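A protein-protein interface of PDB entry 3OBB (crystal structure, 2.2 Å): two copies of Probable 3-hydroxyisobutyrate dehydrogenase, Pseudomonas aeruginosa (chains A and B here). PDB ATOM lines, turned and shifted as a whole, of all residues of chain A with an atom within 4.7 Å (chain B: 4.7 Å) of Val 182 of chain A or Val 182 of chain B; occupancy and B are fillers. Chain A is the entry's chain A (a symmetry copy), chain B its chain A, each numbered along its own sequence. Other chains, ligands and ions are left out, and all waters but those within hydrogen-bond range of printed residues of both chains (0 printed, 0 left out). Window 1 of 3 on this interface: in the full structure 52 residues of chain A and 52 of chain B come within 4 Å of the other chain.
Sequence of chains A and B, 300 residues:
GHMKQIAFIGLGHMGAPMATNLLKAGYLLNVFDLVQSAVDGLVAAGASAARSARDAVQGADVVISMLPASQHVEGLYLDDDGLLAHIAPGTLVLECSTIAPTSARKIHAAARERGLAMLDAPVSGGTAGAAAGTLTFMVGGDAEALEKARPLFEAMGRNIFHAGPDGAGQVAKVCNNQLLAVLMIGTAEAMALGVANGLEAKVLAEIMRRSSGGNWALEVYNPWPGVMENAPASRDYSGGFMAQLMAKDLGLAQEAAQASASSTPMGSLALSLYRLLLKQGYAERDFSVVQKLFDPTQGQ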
ATOM      1  N   GLN A 178      31.067 -34.137 -15.586  1.00  0.00           N
ATOM      2  CA  GLN A 178      30.447 -32.833 -15.425  1.00  0.00           C
ATOM      3  C   GLN A 178      30.162 -32.163 -16.784  1.00  0.00           C
ATOM      4  O   GLN A 178      29.101 -31.549 -16.998  1.00  0.00           O
ATOM      5  CB  GLN A 178      31.279 -31.915 -14.543  1.00  0.00           C
ATOM      6  CG  GLN A 178      30.555 -30.601 -14.262  1.00  0.00           C
ATOM      7  CD  GLN A 178      31.321 -29.699 -13.283  1.00  0.00           C
ATOM      8  OE1 GLN A 178      32.472 -29.314 -13.541  1.00  0.00           O
ATOM      9  NE2 GLN A 178      30.683 -29.351 -12.181  1.00  0.00           N
ATOM     10  N   LEU A 179      31.126 -32.270 -17.696  1.00  0.00           N
ATOM     11  CA  LEU A 179      30.932 -31.763 -19.035  1.00  0.00           C
ATOM     12  C   LEU A 179      29.764 -32.515 -19.752  1.00  0.00           C
ATOM     13  O   LEU A 179      28.943 -31.893 -20.423  1.00  0.00           O
ATOM     14  CB  LEU A 179      32.235 -31.797 -19.846  1.00  0.00           C
ATOM     15  CG  LEU A 179      32.118 -31.299 -21.299  1.00  0.00           C
ATOM     16  CD1 LEU A 179      31.502 -29.875 -21.412  1.00  0.00           C
ATOM     17  CD2 LEU A 179      33.484 -31.275 -21.941  1.00  0.00           C
ATOM     18  N   LEU A 180      29.696 -33.830 -19.582  1.00  0.00           N
ATOM     19  CA  LEU A 180      28.567 -34.612 -20.124  1.00  0.00           C
ATOM     20  C   LEU A 180      27.206 -34.099 -19.634  1.00  0.00           C
ATOM     21  O   LEU A 180      26.248 -34.027 -20.411  1.00  0.00           O
ATOM     22  CB  LEU A 180      28.680 -36.090 -19.728  1.00  0.00           C
ATOM     23  CG  LEU A 180      27.480 -37.017 -20.007  1.00  0.00           C
ATOM     24  CD1 LEU A 180      26.996 -36.965 -21.438  1.00  0.00           C
ATOM     25  CD2 LEU A 180      27.725 -38.520 -19.519  1.00  0.00           C
ATOM     26  N   ALA A 181      27.131 -33.747 -18.358  1.00  0.00           N
ATOM     27  CA  ALA A 181      25.885 -33.320 -17.782  1.00  0.00           C
ATOM     28  C   ALA A 181      25.488 -32.014 -18.431  1.00  0.00           C
ATOM     29  O   ALA A 181      24.342 -31.806 -18.793  1.00  0.00           O
ATOM     30  CB  ALA A 181      26.010 -33.149 -16.249  1.00  0.00           C
ATOM     31  N   VAL A 182      26.451 -31.113 -18.562  1.00  0.00           N
ATOM     32  CA  VAL A 182      26.231 -29.821 -19.216  1.00  0.00           C
ATOM     33  C   VAL A 182      25.789 -30.023 -20.653  1.00  0.00           C
ATOM     34  O   VAL A 182      24.818 -29.391 -21.085  1.00  0.00           O
ATOM     35  CB  VAL A 182      27.523 -29.018 -19.166  1.00  0.00           C
ATOM     36  CG1 VAL A 182      27.505 -27.820 -20.128  1.00  0.00           C
ATOM     37  CG2 VAL A 182      27.825 -28.648 -17.690  1.00  0.00           C
ATOM     38  N   LEU A 183      26.472 -30.901 -21.414  1.00  0.00           N
ATOM     39  CA  LEU A 183      26.046 -31.038 -22.805  1.00  0.00           C
ATOM     40  C   LEU A 183      24.694 -31.720 -22.958  1.00  0.00           C
ATOM     41  O   LEU A 183      23.958 -31.442 -23.923  1.00  0.00           O
ATOM     42  CB  LEU A 183      27.125 -31.663 -23.720  1.00  0.00           C
ATOM     43  CG  LEU A 183      27.618 -33.027 -23.418  1.00  0.00           C
ATOM     44  CD1 LEU A 183      26.646 -34.029 -24.083  1.00  0.00           C
ATOM     45  CD2 LEU A 183      29.079 -33.159 -23.947  1.00  0.00           C
ATOM     46  N   MET A 184      24.379 -32.590 -22.008  1.00  0.00           N
ATOM     47  CA  MET A 184      23.085 -33.272 -21.999  1.00  0.00           C
ATOM     48  C   MET A 184      21.917 -32.309 -21.686  1.00  0.00           C
ATOM     49  O   MET A 184      20.857 -32.320 -22.344  1.00  0.00           O
ATOM     50  CB  MET A 184      23.079 -34.489 -21.052  1.00  0.00           C
ATOM     51  CG  MET A 184      21.716 -35.188 -20.982  1.00  0.00           C
ATOM     52  SD  MET A 184      21.200 -36.024 -22.696  1.00  0.00           S
ATOM     53  CE  MET A 184      22.327 -37.587 -22.708  1.00  0.00           C
ATOM     54  N   ILE A 185      22.103 -31.439 -20.714  1.00  0.00           N
ATOM     55  CA  ILE A 185      21.032 -30.470 -20.438  1.00  0.00           C
ATOM     56  C   ILE A 185      20.947 -29.453 -21.562  1.00  0.00           C
ATOM     57  O   ILE A 185      19.850 -29.115 -22.026  1.00  0.00           O
ATOM     58  CB  ILE A 185      21.220 -29.792 -19.068  1.00  0.00           C
ATOM     59  CG1 ILE A 185      21.309 -30.880 -17.994  1.00  0.00           C
ATOM     60  CG2 ILE A 185      20.037 -28.840 -18.771  1.00  0.00           C
ATOM     61  CD1 ILE A 185      21.444 -30.332 -16.571  1.00  0.00           C
ATOM     62  N   GLY A 186      22.117 -28.984 -22.017  1.00  0.00           N
ATOM     63  CA  GLY A 186      22.190 -28.124 -23.177  1.00  0.00           C
ATOM     64  C   GLY A 186      21.393 -28.734 -24.324  1.00  0.00           C
ATOM     65  O   GLY A 186      20.561 -28.062 -24.925  1.00  0.00           O
ATOM     66  N   GLU A 189      17.498 -28.929 -23.695  1.00  0.00           N
ATOM     67  CA  GLU A 189      16.868 -27.621 -23.715  1.00  0.00           C
ATOM     68  C   GLU A 189      16.801 -27.075 -25.149  1.00  0.00           C
ATOM     69  O   GLU A 189      15.835 -26.372 -25.509  1.00  0.00           O
ATOM     70  CB  GLU A 189      17.606 -26.650 -22.772  1.00  0.00           C
ATOM     71  CG  GLU A 189      18.638 -25.778 -23.417  1.00  0.00           C
ATOM     72  CD  GLU A 189      19.323 -24.804 -22.404  1.00  0.00           C
ATOM     73  OE1 GLU A 189      19.049 -24.898 -21.183  1.00  0.00           O
ATOM     74  OE2 GLU A 189      20.114 -23.943 -22.862  1.00  0.00           O
ATOM     75  N   MET A 266      28.330 -23.754 -15.138  1.00  0.00           N
ATOM     76  CA  MET A 266      27.455 -24.648 -15.897  1.00  0.00           C
ATOM     77  C   MET A 266      27.255 -25.943 -15.144  1.00  0.00           C
ATOM     78  O   MET A 266      26.120 -26.353 -14.959  1.00  0.00           O
ATOM     79  CB  MET A 266      27.967 -24.899 -17.335  1.00  0.00           C
ATOM     80  CG  MET A 266      28.526 -23.670 -17.996  1.00  0.00           C
ATOM     81  SD  MET A 266      27.164 -22.276 -18.360  1.00  0.00           S
ATOM     82  CE  MET A 266      25.907 -23.505 -19.047  1.00  0.00           C
ATOM     83  N   GLY A 267      28.353 -26.575 -14.712  1.00  0.00           N
ATOM     84  CA  GLY A 267      28.301 -27.822 -13.905  1.00  0.00           C
ATOM     85  C   GLY A 267      27.437 -27.658 -12.647  1.00  0.00           C
ATOM     86  O   GLY A 267      26.515 -28.432 -12.460  1.00  0.00           O
ATOM     87  N   ALA A 270      24.003 -27.487 -13.599  1.00  0.00           N
ATOM     88  CA  ALA A 270      23.578 -28.846 -14.000  1.00  0.00           C
ATOM     89  C   ALA A 270      23.187 -29.629 -12.750  1.00  0.00           C
ATOM     90  O   ALA A 270      22.150 -30.285 -12.718  1.00  0.00           O
ATOM     91  CB  ALA A 270      24.675 -29.577 -14.802  1.00  0.00           C
ATOM     92  N   GLN B 178      23.038 -21.461 -29.559  1.00  0.00           N
ATOM     93  CA  GLN B 178      22.889 -21.482 -28.113  1.00  0.00           C
ATOM     94  C   GLN B 178      23.526 -22.740 -27.490  1.00  0.00           C
ATOM     95  O   GLN B 178      24.185 -22.683 -26.436  1.00  0.00           O
ATOM     96  CB  GLN B 178      21.433 -21.359 -27.692  1.00  0.00           C
ATOM     97  CG  GLN B 178      21.296 -21.238 -26.177  1.00  0.00           C
ATOM     98  CD  GLN B 178      19.846 -21.001 -25.729  1.00  0.00           C
ATOM     99  OE1 GLN B 178      18.953 -21.815 -26.008  1.00  0.00           O
ATOM    100  NE2 GLN B 178      19.619 -19.906 -25.025  1.00  0.00           N
ATOM    101  N   LEU B 179      23.311 -23.881 -28.141  1.00  0.00           N
ATOM    102  CA  LEU B 179      23.937 -25.108 -27.703  1.00  0.00           C
ATOM    103  C   LEU B 179      25.494 -25.005 -27.797  1.00  0.00           C
ATOM    104  O   LEU B 179      26.203 -25.439 -26.891  1.00  0.00           O
ATOM    105  CB  LEU B 179      23.384 -26.324 -28.458  1.00  0.00           C
ATOM    106  CG  LEU B 179      24.014 -27.677 -28.075  1.00  0.00           C
ATOM    107  CD1 LEU B 179      23.953 -27.972 -26.548  1.00  0.00           C
ATOM    108  CD2 LEU B 179      23.303 -28.793 -28.801  1.00  0.00           C
ATOM    109  N   LEU B 180      25.997 -24.414 -28.875  1.00  0.00           N
ATOM    110  CA  LEU B 180      27.447 -24.167 -29.003  1.00  0.00           C
ATOM    111  C   LEU B 180      28.011 -23.353 -27.832  1.00  0.00           C
ATOM    112  O   LEU B 180      29.103 -23.648 -27.333  1.00  0.00           O
ATOM    113  CB  LEU B 180      27.764 -23.407 -30.298  1.00  0.00           C
ATOM    114  CG  LEU B 180      29.193 -22.861 -30.495  1.00  0.00           C
ATOM    115  CD1 LEU B 180      30.270 -23.902 -30.303  1.00  0.00           C
ATOM    116  CD2 LEU B 180      29.373 -22.066 -31.872  1.00  0.00           C
ATOM    117  N   ALA B 181      27.269 -22.342 -27.401  1.00  0.00           N
ATOM    118  CA  ALA B 181      27.738 -21.475 -26.356  1.00  0.00           C
ATOM    119  C   ALA B 181      27.835 -22.280 -25.081  1.00  0.00           C
ATOM    120  O   ALA B 181      28.800 -22.186 -24.342  1.00  0.00           O
ATOM    121  CB  ALA B 181      26.788 -20.269 -26.165  1.00  0.00           C
ATOM    122  N   VAL B 182      26.807 -23.073 -24.814  1.00  0.00           N
ATOM    123  CA  VAL B 182      26.779 -23.951 -23.642  1.00  0.00           C
ATOM    124  C   VAL B 182      27.932 -24.936 -23.691  1.00  0.00           C
ATOM    125  O   VAL B 182      28.627 -25.107 -22.682  1.00  0.00           O
ATOM    126  CB  VAL B 182      25.450 -24.692 -23.615  1.00  0.00           C
ATOM    127  CG1 VAL B 182      25.465 -25.887 -22.649  1.00  0.00           C
ATOM    128  CG2 VAL B 182      24.313 -23.670 -23.349  1.00  0.00           C
ATOM    129  N   LEU B 183      28.167 -25.588 -24.846  1.00  0.00           N
ATOM    130  CA  LEU B 183      29.258 -26.560 -24.842  1.00  0.00           C
ATOM    131  C   LEU B 183      30.636 -25.921 -24.744  1.00  0.00           C
ATOM    132  O   LEU B 183      31.573 -26.532 -24.196  1.00  0.00           O
ATOM    133  CB  LEU B 183      29.170 -27.586 -25.995  1.00  0.00           C
ATOM    134  CG  LEU B 183      29.202 -27.098 -27.394  1.00  0.00           C
ATOM    135  CD1 LEU B 183      30.688 -26.952 -27.800  1.00  0.00           C
ATOM    136  CD2 LEU B 183      28.426 -28.108 -28.294  1.00  0.00           C
ATOM    137  N   MET B 184      30.743 -24.703 -25.258  1.00  0.00           N
ATOM    138  CA  MET B 184      31.993 -23.949 -25.177  1.00  0.00           C
ATOM    139  C   MET B 184      32.320 -23.508 -23.732  1.00  0.00           C
ATOM    140  O   MET B 184      33.461 -23.633 -23.244  1.00  0.00           O
ATOM    141  CB  MET B 184      32.012 -22.752 -26.148  1.00  0.00           C
ATOM    142  CG  MET B 184      33.289 -21.912 -26.041  1.00  0.00           C
ATOM    143  SD  MET B 184      34.900 -22.901 -26.614  1.00  0.00           S
ATOM    144  CE  MET B 184      34.698 -22.879 -28.530  1.00  0.00           C
ATOM    145  N   ILE B 185      31.324 -23.028 -23.014  1.00  0.00           N
ATOM    146  CA  ILE B 185      31.593 -22.660 -21.616  1.00  0.00           C
ATOM    147  C   ILE B 185      31.817 -23.909 -20.782  1.00  0.00           C
ATOM    148  O   ILE B 185      32.744 -23.963 -19.963  1.00  0.00           O
ATOM    149  CB  ILE B 185      30.470 -21.781 -21.036  1.00  0.00           C
ATOM    150  CG1 ILE B 185      30.298 -20.553 -21.936  1.00  0.00           C
ATOM    151  CG2 ILE B 185      30.820 -21.342 -19.593  1.00  0.00           C
ATOM    152  CD1 ILE B 185      29.241 -19.564 -21.435  1.00  0.00           C
ATOM    153  N   GLY B 186      30.976 -24.926 -21.014  1.00  0.00           N
ATOM    154  CA  GLY B 186      31.163 -26.221 -20.398  1.00  0.00           C
ATOM    155  C   GLY B 186      32.603 -26.682 -20.592  1.00  0.00           C
ATOM    156  O   GLY B 186      33.264 -27.068 -19.633  1.00  0.00           O
ATOM    157  N   GLU B 189      35.297 -24.486 -18.715  1.00  0.00           N
ATOM    158  CA  GLU B 189      35.247 -24.660 -17.275  1.00  0.00           C
ATOM    159  C   GLU B 189      35.809 -26.031 -16.875  1.00  0.00           C
ATOM    160  O   GLU B 189      36.434 -26.166 -15.804  1.00  0.00           O
ATOM    161  CB  GLU B 189      33.808 -24.463 -16.756  1.00  0.00           C
ATOM    162  CG  GLU B 189      33.003 -25.713 -16.585  1.00  0.00           C
ATOM    163  CD  GLU B 189      31.568 -25.436 -16.032  1.00  0.00           C
ATOM    164  OE1 GLU B 189      31.187 -24.249 -15.885  1.00  0.00           O
ATOM    165  OE2 GLU B 189      30.854 -26.424 -15.734  1.00  0.00           O
ATOM    166  N   MET B 266      20.616 -23.245 -19.241  1.00  0.00           N
ATOM    167  CA  MET B 266      22.033 -23.253 -19.609  1.00  0.00           C
ATOM    168  C   MET B 266      22.328 -22.116 -20.562  1.00  0.00           C
ATOM    169  O   MET B 266      23.257 -21.362 -20.317  1.00  0.00           O
ATOM    170  CB  MET B 266      22.488 -24.612 -20.189  1.00  0.00           C
ATOM    171  CG  MET B 266      21.902 -25.797 -19.472  1.00  0.00           C
ATOM    172  SD  MET B 266      22.544 -25.991 -17.606  1.00  0.00           S
ATOM    173  CE  MET B 266      24.348 -25.674 -18.061  1.00  0.00           C
ATOM    174  N   GLY B 267      21.538 -21.996 -21.635  1.00  0.00           N
ATOM    175  CA  GLY B 267      21.673 -20.889 -22.618  1.00  0.00           C
ATOM    176  C   GLY B 267      21.612 -19.511 -21.945  1.00  0.00           C
ATOM    177  O   GLY B 267      22.529 -18.728 -22.121  1.00  0.00           O
ATOM    178  N   ALA B 270      24.620 -18.972 -20.104  1.00  0.00           N
ATOM    179  CA  ALA B 270      25.705 -18.711 -21.077  1.00  0.00           C
ATOM    180  C   ALA B 270      25.678 -17.233 -21.458  1.00  0.00           C
ATOM    181  O   ALA B 270      26.712 -16.573 -21.485  1.00  0.00           O
ATOM    182  CB  ALA B 270      25.588 -19.615 -22.323  1.00  0.00           C
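The backbone NH (N) of Gly 267 of chain B is in hydrogen-bond range of the side-chain carboxylate (OE2) of Glu 189 of chain A (2.7 Å).
The side-chain carboxylate (OE2) of Glu 189 of chain B lies within hydrogen-bond range of the backbone NH (N) of Gly 267 of chain A, at 2.7 Å.
The side-chain carboxylate (OE1) of Glu 189 of chain A is in hydrogen-bond range of the backbone NH (N) of Met 266 of chain B (3.0 Å).
The side-chain carboxylate (OE1) of Glu 189 of chain B lies within hydrogen-bond range of the backbone NH (N) of Met 266 of chain A.
Glu 189 of chain B touches Gln 178 of chain A (OE2 to OE1, 3.97 Å).
CD1 of Leu 179 of chain A touches C of Gly 186 of chain B (3.5 Å).
Val 182 of chain A touches Val 182 of chain B.
Ile 185 of chain A touches Met 266 of chain B.
CD1 of Leu 179 of chain B touches C of Gly 186 of chain A, at 3.5 Å.
Glu 189 of chain A touches Gln 178 of chain B (OE2 to OE1, 3.97 Å).
CG2 of Ile 185 of chain B touches CG of Met 266 of chain A, at 3.6 Å.
Met 266 of chain B touches Met 266 of chain A.
Printed residues of chain B within 4 Å of Gln 178 of chain A: Glu 189.
Of the printed residues of chain B, Val 182 of chain A touches Val 182 (3.8 Å).
Printed residues of chain B within 4 Å of Glu 189 of chain A: Gln 178, Met 266 and Gly 267.
Printed residues of chain A within 4 Å of Gln 178 of chain B: Glu 189 (3.97 Å).
Of the printed residues of chain A, Leu 179 of chain B touches Gly 186 (3.5 Å).
Printed residues of chain A within 4 Å of Val 182 of chain B: Val 182 (3.8 Å).
Val 182 of chain A touches its own counterpart, Val 182 of chain B.
Glu 189 of chain A touches Met 266 of chain B, and with the chains exchanged Met 266 of chain A touches Glu 189 of chain B.
Glu 189 of chain A touches Gly 267 of chain B, and with the chains exchanged Gly 267 of chain A touches Glu 189 of chain B.
Met 266 of chain B touches its own counterpart, Met 266 of chain A.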
